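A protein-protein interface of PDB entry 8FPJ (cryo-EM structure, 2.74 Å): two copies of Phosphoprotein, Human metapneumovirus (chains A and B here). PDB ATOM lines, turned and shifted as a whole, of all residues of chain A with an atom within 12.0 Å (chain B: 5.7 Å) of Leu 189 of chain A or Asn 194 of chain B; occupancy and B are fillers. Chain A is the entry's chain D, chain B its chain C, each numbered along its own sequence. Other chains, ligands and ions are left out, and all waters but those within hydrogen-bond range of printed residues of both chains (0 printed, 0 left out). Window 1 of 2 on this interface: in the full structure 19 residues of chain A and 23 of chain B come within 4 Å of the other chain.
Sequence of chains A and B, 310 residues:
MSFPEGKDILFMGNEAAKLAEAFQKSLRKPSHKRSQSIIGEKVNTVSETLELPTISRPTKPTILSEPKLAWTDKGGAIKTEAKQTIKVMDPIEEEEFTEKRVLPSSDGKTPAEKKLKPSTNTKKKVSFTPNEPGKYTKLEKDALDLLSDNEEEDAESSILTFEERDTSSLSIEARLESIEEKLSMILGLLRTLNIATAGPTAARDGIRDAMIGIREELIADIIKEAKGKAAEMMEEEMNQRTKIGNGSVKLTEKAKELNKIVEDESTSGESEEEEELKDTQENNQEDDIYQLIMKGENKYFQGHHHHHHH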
ATOM      1  N   GLU A 180     -37.183  13.332  23.876  1.00  0.00           N
ATOM      2  CA  GLU A 180     -35.800  13.290  24.339  1.00  0.00           C
ATOM      3  C   GLU A 180     -35.311  11.853  24.484  1.00  0.00           C
ATOM      4  O   GLU A 180     -34.196  11.519  24.064  1.00  0.00           O
ATOM      5  CB  GLU A 180     -35.669  14.037  25.665  1.00  0.00           C
ATOM      6  CG  GLU A 180     -34.282  13.973  26.286  1.00  0.00           C
ATOM      7  CD  GLU A 180     -33.187  14.370  25.318  1.00  0.00           C
ATOM      8  OE1 GLU A 180     -33.259  15.487  24.764  1.00  0.00           O
ATOM      9  OE2 GLU A 180     -32.252  13.568  25.114  1.00  0.00           O
ATOM     10  N   GLU A 181     -36.137  10.984  25.068  1.00  0.00           N
ATOM     11  CA  GLU A 181     -35.742   9.588  25.217  1.00  0.00           C
ATOM     12  C   GLU A 181     -35.551   8.925  23.860  1.00  0.00           C
ATOM     13  O   GLU A 181     -34.597   8.160  23.658  1.00  0.00           O
ATOM     14  CB  GLU A 181     -36.786   8.834  26.039  1.00  0.00           C
ATOM     15  CG  GLU A 181     -36.651   9.046  27.535  1.00  0.00           C
ATOM     16  CD  GLU A 181     -35.571   8.174  28.150  1.00  0.00           C
ATOM     17  OE1 GLU A 181     -35.431   7.007  27.725  1.00  0.00           O
ATOM     18  OE2 GLU A 181     -34.859   8.657  29.055  1.00  0.00           O
ATOM     19  N   LYS A 182     -36.457   9.192  22.918  1.00  0.00           N
ATOM     20  CA  LYS A 182     -36.340   8.580  21.601  1.00  0.00           C
ATOM     21  C   LYS A 182     -35.080   9.050  20.888  1.00  0.00           C
ATOM     22  O   LYS A 182     -34.408   8.259  20.220  1.00  0.00           O
ATOM     23  CB  LYS A 182     -37.585   8.875  20.771  1.00  0.00           C
ATOM     24  CG  LYS A 182     -38.834   8.130  21.229  1.00  0.00           C
ATOM     25  CD  LYS A 182     -40.064   8.595  20.468  1.00  0.00           C
ATOM     26  CE  LYS A 182     -41.336   7.970  20.989  1.00  0.00           C
ATOM     27  NZ  LYS A 182     -42.303   7.737  19.884  1.00  0.00           N
ATOM     28  N   LEU A 183     -34.733  10.333  21.019  1.00  0.00           N
ATOM     29  CA  LEU A 183     -33.464  10.793  20.458  1.00  0.00           C
ATOM     30  C   LEU A 183     -32.274  10.144  21.152  1.00  0.00           C
ATOM     31  O   LEU A 183     -31.245   9.896  20.511  1.00  0.00           O
ATOM     32  CB  LEU A 183     -33.355  12.315  20.542  1.00  0.00           C
ATOM     33  CG  LEU A 183     -34.341  13.112  19.689  1.00  0.00           C
ATOM     34  CD1 LEU A 183     -34.207  14.594  19.978  1.00  0.00           C
ATOM     35  CD2 LEU A 183     -34.115  12.838  18.211  1.00  0.00           C
ATOM     36  N   SER A 184     -32.378   9.874  22.454  1.00  0.00           N
ATOM     37  CA  SER A 184     -31.296   9.166  23.131  1.00  0.00           C
ATOM     38  C   SER A 184     -31.104   7.769  22.547  1.00  0.00           C
ATOM     39  O   SER A 184     -29.971   7.346  22.289  1.00  0.00           O
ATOM     40  CB  SER A 184     -31.577   9.086  24.631  1.00  0.00           C
ATOM     41  OG  SER A 184     -31.345  10.335  25.257  1.00  0.00           O
ATOM     42  N   MET A 185     -32.201   7.039  22.324  1.00  0.00           N
ATOM     43  CA  MET A 185     -32.063   5.739  21.668  1.00  0.00           C
ATOM     44  C   MET A 185     -31.569   5.881  20.234  1.00  0.00           C
ATOM     45  O   MET A 185     -30.861   5.000  19.737  1.00  0.00           O
ATOM     46  CB  MET A 185     -33.370   4.938  21.687  1.00  0.00           C
ATOM     47  CG  MET A 185     -33.694   4.277  23.024  1.00  0.00           C
ATOM     48  SD  MET A 185     -34.259   5.364  24.334  1.00  0.00           S
ATOM     49  CE  MET A 185     -35.920   5.677  23.743  1.00  0.00           C
ATOM     50  N   ILE A 186     -31.931   6.966  19.548  1.00  0.00           N
ATOM     51  CA  ILE A 186     -31.416   7.190  18.199  1.00  0.00           C
ATOM     52  C   ILE A 186     -29.899   7.305  18.236  1.00  0.00           C
ATOM     53  O   ILE A 186     -29.187   6.684  17.437  1.00  0.00           O
ATOM     54  CB  ILE A 186     -32.056   8.444  17.576  1.00  0.00           C
ATOM     55  CG1 ILE A 186     -33.482   8.141  17.116  1.00  0.00           C
ATOM     56  CG2 ILE A 186     -31.218   8.947  16.407  1.00  0.00           C
ATOM     57  CD1 ILE A 186     -34.337   9.363  16.896  1.00  0.00           C
ATOM     58  N   LEU A 187     -29.384   8.103  19.172  1.00  0.00           N
ATOM     59  CA  LEU A 187     -27.939   8.239  19.314  1.00  0.00           C
ATOM     60  C   LEU A 187     -27.297   6.904  19.666  1.00  0.00           C
ATOM     61  O   LEU A 187     -26.238   6.556  19.132  1.00  0.00           O
ATOM     62  CB  LEU A 187     -27.612   9.287  20.379  1.00  0.00           C
ATOM     63  CG  LEU A 187     -27.368  10.712  19.880  1.00  0.00           C
ATOM     64  CD1 LEU A 187     -27.194  11.663  21.054  1.00  0.00           C
ATOM     65  CD2 LEU A 187     -26.157  10.770  18.962  1.00  0.00           C
ATOM     66  N   GLY A 188     -27.922   6.144  20.566  1.00  0.00           N
ATOM     67  CA  GLY A 188     -27.379   4.840  20.915  1.00  0.00           C
ATOM     68  C   GLY A 188     -27.279   3.913  19.718  1.00  0.00           C
ATOM     69  O   GLY A 188     -26.254   3.262  19.505  1.00  0.00           O
ATOM     70  N   LEU A 189     -28.348   3.843  18.920  1.00  0.00           N
ATOM     71  CA  LEU A 189     -28.324   3.012  17.719  1.00  0.00           C
ATOM     72  C   LEU A 189     -27.258   3.480  16.742  1.00  0.00           C
ATOM     73  O   LEU A 189     -26.515   2.665  16.185  1.00  0.00           O
ATOM     74  CB  LEU A 189     -29.695   3.024  17.041  1.00  0.00           C
ATOM     75  CG  LEU A 189     -30.734   2.007  17.509  1.00  0.00           C
ATOM     76  CD1 LEU A 189     -32.053   2.250  16.804  1.00  0.00           C
ATOM     77  CD2 LEU A 189     -30.251   0.593  17.244  1.00  0.00           C
ATOM     78  N   LEU A 190     -27.166   4.792  16.517  1.00  0.00           N
ATOM     79  CA  LEU A 190     -26.239   5.308  15.518  1.00  0.00           C
ATOM     80  C   LEU A 190     -24.787   5.042  15.890  1.00  0.00           C
ATOM     81  O   LEU A 190     -23.913   5.114  15.020  1.00  0.00           O
ATOM     82  CB  LEU A 190     -26.465   6.809  15.331  1.00  0.00           C
ATOM     83  CG  LEU A 190     -26.192   7.383  13.941  1.00  0.00           C
ATOM     84  CD1 LEU A 190     -27.058   6.710  12.891  1.00  0.00           C
ATOM     85  CD2 LEU A 190     -26.425   8.881  13.945  1.00  0.00           C
ATOM     86  N   ARG A 191     -24.512   4.738  17.159  1.00  0.00           N
ATOM     87  CA  ARG A 191     -23.149   4.454  17.587  1.00  0.00           C
ATOM     88  C   ARG A 191     -22.672   3.081  17.130  1.00  0.00           C
ATOM     89  O   ARG A 191     -21.518   2.938  16.713  1.00  0.00           O
ATOM     90  CB  ARG A 191     -23.056   4.554  19.109  1.00  0.00           C
ATOM     91  CG  ARG A 191     -21.658   4.775  19.636  1.00  0.00           C
ATOM     92  CD  ARG A 191     -21.679   5.676  20.854  1.00  0.00           C
ATOM     93  NE  ARG A 191     -22.018   7.051  20.507  1.00  0.00           N
ATOM     94  CZ  ARG A 191     -22.101   8.046  21.379  1.00  0.00           C
ATOM     95  NH1 ARG A 191     -21.877   7.855  22.669  1.00  0.00           N
ATOM     96  NH2 ARG A 191     -22.416   9.262  20.946  1.00  0.00           N
ATOM     97  N   THR A 192     -23.532   2.068  17.206  1.00  0.00           N
ATOM     98  CA  THR A 192     -23.169   0.711  16.821  1.00  0.00           C
ATOM     99  C   THR A 192     -23.163   0.497  15.314  1.00  0.00           C
ATOM    100  O   THR A 192     -22.552  -0.468  14.845  1.00  0.00           O
ATOM    101  CB  THR A 192     -24.138  -0.290  17.459  1.00  0.00           C
ATOM    102  OG1 THR A 192     -24.391   0.081  18.819  1.00  0.00           O
ATOM    103  CG2 THR A 192     -23.562  -1.694  17.421  1.00  0.00           C
ATOM    104  N   LEU A 193     -23.815   1.370  14.544  1.00  0.00           N
ATOM    105  CA  LEU A 193     -23.965   1.147  13.112  1.00  0.00           C
ATOM    106  C   LEU A 193     -22.669   1.337  12.337  1.00  0.00           C
ATOM    107  O   LEU A 193     -22.632   0.998  11.149  1.00  0.00           O
ATOM    108  CB  LEU A 193     -25.035   2.085  12.548  1.00  0.00           C
ATOM    109  CG  LEU A 193     -26.495   1.737  12.846  1.00  0.00           C
ATOM    110  CD1 LEU A 193     -27.413   2.709  12.136  1.00  0.00           C
ATOM    111  CD2 LEU A 193     -26.819   0.312  12.441  1.00  0.00           C
ATOM    112  N   ASN A 194     -21.615   1.862  12.960  1.00  0.00           N
ATOM    113  CA  ASN A 194     -20.371   2.106  12.241  1.00  0.00           C
ATOM    114  C   ASN A 194     -19.246   1.232  12.782  1.00  0.00           C
ATOM    115  O   ASN A 194     -18.104   1.682  12.903  1.00  0.00           O
ATOM    116  CB  ASN A 194     -19.986   3.585  12.321  1.00  0.00           C
ATOM    117  CG  ASN A 194     -20.111   4.143  13.718  1.00  0.00           C
ATOM    118  OD1 ASN A 194     -20.091   3.402  14.698  1.00  0.00           O
ATOM    119  ND2 ASN A 194     -20.246   5.460  13.819  1.00  0.00           N
ATOM    120  N   ILE A 195     -19.567  -0.022  13.105  1.00  0.00           N
ATOM    121  CA  ILE A 195     -18.578  -1.019  13.485  1.00  0.00           C
ATOM    122  C   ILE A 195     -18.544  -2.180  12.500  1.00  0.00           C
ATOM    123  O   ILE A 195     -17.507  -2.833  12.337  1.00  0.00           O
ATOM    124  CB  ILE A 195     -18.832  -1.541  14.916  1.00  0.00           C
ATOM    125  CG1 ILE A 195     -18.982  -0.380  15.906  1.00  0.00           C
ATOM    126  CG2 ILE A 195     -17.706  -2.465  15.350  1.00  0.00           C
ATOM    127  CD1 ILE A 195     -17.778   0.534  15.983  1.00  0.00           C
ATOM    128  N   ALA A 196     -19.665  -2.455  11.831  1.00  0.00           N
ATOM    129  CA  ALA A 196     -19.735  -3.604  10.935  1.00  0.00           C
ATOM    130  C   ALA A 196     -19.142  -3.276   9.569  1.00  0.00           C
ATOM    131  O   ALA A 196     -18.163  -3.896   9.139  1.00  0.00           O
ATOM    132  CB  ALA A 196     -21.186  -4.066  10.795  1.00  0.00           C
ATOM    133  N   THR A 197     -19.722  -2.303   8.871  1.00  0.00           N
ATOM    134  CA  THR A 197     -19.290  -1.954   7.523  1.00  0.00           C
ATOM    135  C   THR A 197     -18.544  -0.627   7.460  1.00  0.00           C
ATOM    136  O   THR A 197     -17.527  -0.529   6.768  1.00  0.00           O
ATOM    137  CB  THR A 197     -20.493  -1.910   6.570  1.00  0.00           C
ATOM    138  OG1 THR A 197     -20.041  -1.633   5.238  1.00  0.00           O
ATOM    139  CG2 THR A 197     -21.498  -0.843   6.993  1.00  0.00           C
ATOM    140  N   ALA A 198     -19.020   0.400   8.169  1.00  0.00           N
ATOM    141  CA  ALA A 198     -18.345   1.692   8.125  1.00  0.00           C
ATOM    142  C   ALA A 198     -17.048   1.678   8.924  1.00  0.00           C
ATOM    143  O   ALA A 198     -16.178   2.527   8.703  1.00  0.00           O
ATOM    144  CB  ALA A 198     -19.272   2.791   8.644  1.00  0.00           C
ATOM    145  N   GLY A 199     -16.901   0.733   9.849  1.00  0.00           N
ATOM    146  CA  GLY A 199     -15.699   0.629  10.641  1.00  0.00           C
ATOM    147  C   GLY A 199     -14.641  -0.212   9.955  1.00  0.00           C
ATOM    148  O   GLY A 199     -14.947  -1.089   9.140  1.00  0.00           O
ATOM    149  N   ARG A 204     -12.183  -4.327  13.880  1.00  0.00           N
ATOM    150  CA  ARG A 204     -13.383  -5.156  13.903  1.00  0.00           C
ATOM    151  C   ARG A 204     -13.300  -6.238  14.972  1.00  0.00           C
ATOM    152  O   ARG A 204     -14.334  -6.692  15.475  1.00  0.00           O
ATOM    153  CB  ARG A 204     -13.590  -5.781  12.523  1.00  0.00           C
ATOM    154  CG  ARG A 204     -14.879  -6.554  12.351  1.00  0.00           C
ATOM    155  CD  ARG A 204     -14.919  -7.227  10.987  1.00  0.00           C
ATOM    156  NE  ARG A 204     -14.963  -6.265   9.893  1.00  0.00           N
ATOM    157  CZ  ARG A 204     -16.073  -5.731   9.405  1.00  0.00           C
ATOM    158  NH1 ARG A 204     -17.262  -6.033   9.900  1.00  0.00           N
ATOM    159  NH2 ARG A 204     -15.988  -4.869   8.396  1.00  0.00           N
ATOM    160  N   ILE A 207     -13.815  -5.873  19.944  1.00  0.00           N
ATOM    161  CA  ILE A 207     -14.860  -6.218  20.901  1.00  0.00           C
ATOM    162  C   ILE A 207     -14.857  -7.703  21.242  1.00  0.00           C
ATOM    163  O   ILE A 207     -15.431  -8.099  22.265  1.00  0.00           O
ATOM    164  CB  ILE A 207     -16.240  -5.792  20.365  1.00  0.00           C
ATOM    165  CG1 ILE A 207     -16.257  -4.295  20.041  1.00  0.00           C
ATOM    166  CG2 ILE A 207     -17.329  -6.129  21.373  1.00  0.00           C
ATOM    167  CD1 ILE A 207     -17.460  -3.860  19.230  1.00  0.00           C
ATOM    168  N   LEU B 187     -36.298   5.707  14.045  1.00  0.00           N
ATOM    169  CA  LEU B 187     -35.849   4.689  14.989  1.00  0.00           C
ATOM    170  C   LEU B 187     -36.076   3.286  14.437  1.00  0.00           C
ATOM    171  O   LEU B 187     -35.202   2.417  14.544  1.00  0.00           O
ATOM    172  CB  LEU B 187     -36.578   4.869  16.320  1.00  0.00           C
ATOM    173  CG  LEU B 187     -35.899   4.395  17.603  1.00  0.00           C
ATOM    174  CD1 LEU B 187     -34.568   5.073  17.835  1.00  0.00           C
ATOM    175  CD2 LEU B 187     -36.821   4.654  18.776  1.00  0.00           C
ATOM    176  N   LEU B 189     -36.296   2.512  11.235  1.00  0.00           N
ATOM    177  CA  LEU B 189     -35.367   2.354  10.118  1.00  0.00           C
ATOM    178  C   LEU B 189     -33.975   1.976  10.614  1.00  0.00           C
ATOM    179  O   LEU B 189     -33.322   1.084  10.058  1.00  0.00           O
ATOM    180  CB  LEU B 189     -35.317   3.640   9.290  1.00  0.00           C
ATOM    181  CG  LEU B 189     -36.526   3.900   8.385  1.00  0.00           C
ATOM    182  CD1 LEU B 189     -36.661   5.376   8.066  1.00  0.00           C
ATOM    183  CD2 LEU B 189     -36.424   3.093   7.104  1.00  0.00           C
ATOM    184  N   LEU B 190     -33.508   2.639  11.676  1.00  0.00           N
ATOM    185  CA  LEU B 190     -32.185   2.343  12.213  1.00  0.00           C
ATOM    186  C   LEU B 190     -32.137   0.961  12.852  1.00  0.00           C
ATOM    187  O   LEU B 190     -31.116   0.272  12.771  1.00  0.00           O
ATOM    188  CB  LEU B 190     -31.773   3.410  13.225  1.00  0.00           C
ATOM    189  CG  LEU B 190     -31.503   4.803  12.659  1.00  0.00           C
ATOM    190  CD1 LEU B 190     -31.359   5.811  13.787  1.00  0.00           C
ATOM    191  CD2 LEU B 190     -30.268   4.803  11.777  1.00  0.00           C
ATOM    192  N   ARG B 191     -33.225   0.537  13.497  1.00  0.00           N
ATOM    193  CA  ARG B 191     -33.277  -0.821  14.033  1.00  0.00           C
ATOM    194  C   ARG B 191     -33.095  -1.850  12.925  1.00  0.00           C
ATOM    195  O   ARG B 191     -32.281  -2.777  13.043  1.00  0.00           O
ATOM    196  CB  ARG B 191     -34.605  -1.044  14.757  1.00  0.00           C
ATOM    197  CG  ARG B 191     -34.684  -2.345  15.540  1.00  0.00           C
ATOM    198  CD  ARG B 191     -33.922  -2.250  16.844  1.00  0.00           C
ATOM    199  NE  ARG B 191     -34.528  -1.288  17.755  1.00  0.00           N
ATOM    200  CZ  ARG B 191     -33.947  -0.834  18.856  1.00  0.00           C
ATOM    201  NH1 ARG B 191     -32.735  -1.227  19.212  1.00  0.00           N
ATOM    202  NH2 ARG B 191     -34.598   0.041  19.618  1.00  0.00           N
ATOM    203  N   THR B 192     -33.849  -1.702  11.833  1.00  0.00           N
ATOM    204  CA  THR B 192     -33.716  -2.654  10.734  1.00  0.00           C
ATOM    205  C   THR B 192     -32.317  -2.605  10.130  1.00  0.00           C
ATOM    206  O   THR B 192     -31.731  -3.648   9.811  1.00  0.00           O
ATOM    207  CB  THR B 192     -34.776  -2.381   9.669  1.00  0.00           C
ATOM    208  OG1 THR B 192     -36.074  -2.411  10.271  1.00  0.00           O
ATOM    209  CG2 THR B 192     -34.713  -3.427   8.568  1.00  0.00           C
ATOM    210  N   LEU B 193     -31.760  -1.401   9.972  1.00  0.00           N
ATOM    211  CA  LEU B 193     -30.415  -1.280   9.421  1.00  0.00           C
ATOM    212  C   LEU B 193     -29.393  -1.985  10.303  1.00  0.00           C
ATOM    213  O   LEU B 193     -28.496  -2.672   9.802  1.00  0.00           O
ATOM    214  CB  LEU B 193     -30.050   0.194   9.256  1.00  0.00           C
ATOM    215  CG  LEU B 193     -28.686   0.496   8.632  1.00  0.00           C
ATOM    216  CD1 LEU B 193     -28.562  -0.146   7.263  1.00  0.00           C
ATOM    217  CD2 LEU B 193     -28.466   1.992   8.542  1.00  0.00           C
ATOM    218  N   ASN B 194     -29.506  -1.820  11.622  1.00  0.00           N
ATOM    219  CA  ASN B 194     -28.576  -2.476  12.534  1.00  0.00           C
ATOM    220  C   ASN B 194     -28.705  -3.992  12.460  1.00  0.00           C
ATOM    221  O   ASN B 194     -27.695  -4.704  12.455  1.00  0.00           O
ATOM    222  CB  ASN B 194     -28.812  -1.989  13.962  1.00  0.00           C
ATOM    223  CG  ASN B 194     -27.624  -2.236  14.866  1.00  0.00           C
ATOM    224  OD1 ASN B 194     -26.581  -2.712  14.423  1.00  0.00           O
ATOM    225  ND2 ASN B 194     -27.776  -1.915  16.142  1.00  0.00           N
ATOM    226  N   ILE B 195     -29.934  -4.510  12.404  1.00  0.00           N
ATOM    227  CA  ILE B 195     -30.094  -5.957  12.276  1.00  0.00           C
ATOM    228  C   ILE B 195     -29.448  -6.449  10.986  1.00  0.00           C
ATOM    229  O   ILE B 195     -28.805  -7.504  10.962  1.00  0.00           O
ATOM    230  CB  ILE B 195     -31.581  -6.358  12.345  1.00  0.00           C
ATOM    231  CG1 ILE B 195     -32.219  -5.921  13.665  1.00  0.00           C
ATOM    232  CG2 ILE B 195     -31.725  -7.861  12.170  1.00  0.00           C
ATOM    233  CD1 ILE B 195     -31.595  -6.535  14.895  1.00  0.00           C
ATOM    234  N   ALA B 196     -29.606  -5.696   9.894  1.00  0.00           N
ATOM    235  CA  ALA B 196     -29.175  -6.190   8.588  1.00  0.00           C
ATOM    236  C   ALA B 196     -27.656  -6.302   8.483  1.00  0.00           C
ATOM    237  O   ALA B 196     -27.144  -7.238   7.861  1.00  0.00           O
ATOM    238  CB  ALA B 196     -29.713  -5.282   7.486  1.00  0.00           C
ATOM    239  N   THR B 197     -26.918  -5.361   9.068  1.00  0.00           N
ATOM    240  CA  THR B 197     -25.479  -5.263   8.846  1.00  0.00           C
ATOM    241  C   THR B 197     -24.651  -6.170   9.751  1.00  0.00           C
ATOM    242  O   THR B 197     -23.433  -6.251   9.566  1.00  0.00           O
ATOM    243  CB  THR B 197     -25.016  -3.816   9.030  1.00  0.00           C
ATOM    244  OG1 THR B 197     -25.502  -3.310  10.277  1.00  0.00           O
ATOM    245  CG2 THR B 197     -25.522  -2.946   7.896  1.00  0.00           C
ATOM    246  N   ALA B 198     -25.265  -6.850  10.713  1.00  0.00           N
ATOM    247  CA  ALA B 198     -24.564  -7.766  11.612  1.00  0.00           C
ATOM    248  C   ALA B 198     -24.810  -9.186  11.106  1.00  0.00           C
ATOM    249  O   ALA B 198     -25.732  -9.866  11.556  1.00  0.00           O
ATOM    250  CB  ALA B 198     -25.040  -7.590  13.049  1.00  0.00           C
ATOM    251  N   MET B 211     -23.474  -6.324  18.883  1.00  0.00           N
ATOM    252  CA  MET B 211     -24.331  -5.503  18.036  1.00  0.00           C
ATOM    253  C   MET B 211     -25.802  -5.693  18.381  1.00  0.00           C
ATOM    254  O   MET B 211     -26.572  -4.726  18.379  1.00  0.00           O
ATOM    255  CB  MET B 211     -24.084  -5.832  16.565  1.00  0.00           C
ATOM    256  CG  MET B 211     -22.872  -5.133  15.976  1.00  0.00           C
ATOM    257  SD  MET B 211     -22.418  -5.762  14.352  1.00  0.00           S
ATOM    258  CE  MET B 211     -20.642  -5.548  14.401  1.00  0.00           C
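The backbone carbonyl oxygen (O) of Leu 193 of chain B sits at hydrogen-bond distance from the side-chain hydroxyl (OG1) of Thr 197 of chain B (3.1 Å).
O of Ala 196 of chain A lies within hydrogen-bond range of NH1 of Arg 204 of chain A (2.4 Å).
OG1 of Thr 197 of chain B lies within hydrogen-bond range of O of Asn 194 of chain B (3.4 Å).
Among the printed residues, merely in contact across the chains: Lys 182 of chain A with Leu 187 of chain B, Met 185 of chain A with Leu 187 of chain B, Ile 186 of chain A with Leu 187 of chain B, Leu 189 of chain A with Leu 187 of chain B, Leu 189 of chain A with Leu 190 of chain B, Leu 189 of chain A with Arg 191 of chain B, Leu 189 of chain A with Asn 194 of chain B, Leu 190 of chain A with Leu 190 of chain B, Thr 192 of chain A with Met 211 of chain B, Leu 193 of chain A with Leu 190 of chain B, Leu 193 of chain A with Leu 193 of chain B, Leu 193 of chain A with Asn 194 of chain B, Ala 196 of chain A with Thr 197 of chain B and Ala 196 of chain A with Met 211 of chain B.
Of the printed residues of chain B, Lys 182 of chain A touches Leu 187.
Gly 188 of chain A touches none of the printed residues of chain B.
Of the printed residues of chain B, Leu 189 of chain A touches Leu 187, Leu 190, Arg 191 and Asn 194.
Printed residues of chain B within 4 Å of Leu 190 of chain A: Leu 190.
Leu 189 of chain B touches none of the printed residues of chain A.
Leu 190 of chain B touches three residues of chain A.
Thr 192 of chain B touches none of the printed residues of chain A.
Of chain A, only Leu 193 comes within 4 Å of Leu 193 of chain B.
Of chain A, only Leu 189 (3.7 Å) and Leu 193 (3.3 Å) come within 4 Å of Asn 194 of chain B.
No residue of chain A comes within 4 Å of Ile 195 of chain B.
No residue of chain A comes within 4 Å of Ala 196 of chain B.
Of chain A, only Ala 196 (3.4 Å) comes within 4 Å of Thr 197 of chain B.
Of chain A, only Thr 192 (3.8 Å) and Ala 196 (3.9 Å) come within 4 Å of Met 211 of chain B.
The nearest printed residue of chain A that does not touch Leu 187 of chain B is Leu 183 of chain A (6.2 Å).
Of the 12 printed residues of chain B, 7 touch a printed residue of chain A.
Hydrophobic or aromatic side chains of chain A within 4 Å of the printed part of chain B: Ile 186, Leu 189, Leu 190, Leu 193 and Ala 196.
Among the printed residues, 14 pairs touch across the chains.
Among the printed residues, no Asp or Glu carboxylate lies within 4 Å of a Lys or Arg side-chain nitrogen of the other chain.
Leu 193 of chain A touches Leu 190 of chain B, but with the chains exchanged Leu 190 of chain A does not touch Leu 193 of chain B (6.6 Å).
Leu 193 of chain B touches its own counterpart, Leu 193 of chain A.
Leu 193 of chain A touches Asn 194 of chain B, but with the chains exchanged Asn 194 of chain A does not touch Leu 193 of chain B (8.2 Å).
Ala 196 of chain A touches Thr 197 of chain B, but with the chains exchanged Thr 197 of chain A does not touch Ala 196 of chain B (8.4 Å).
11 positions are printed for both chains.
Of the 14 pairs that touch across the chains among the printed residues, 2 have their exchanged pair printed and touching as well.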
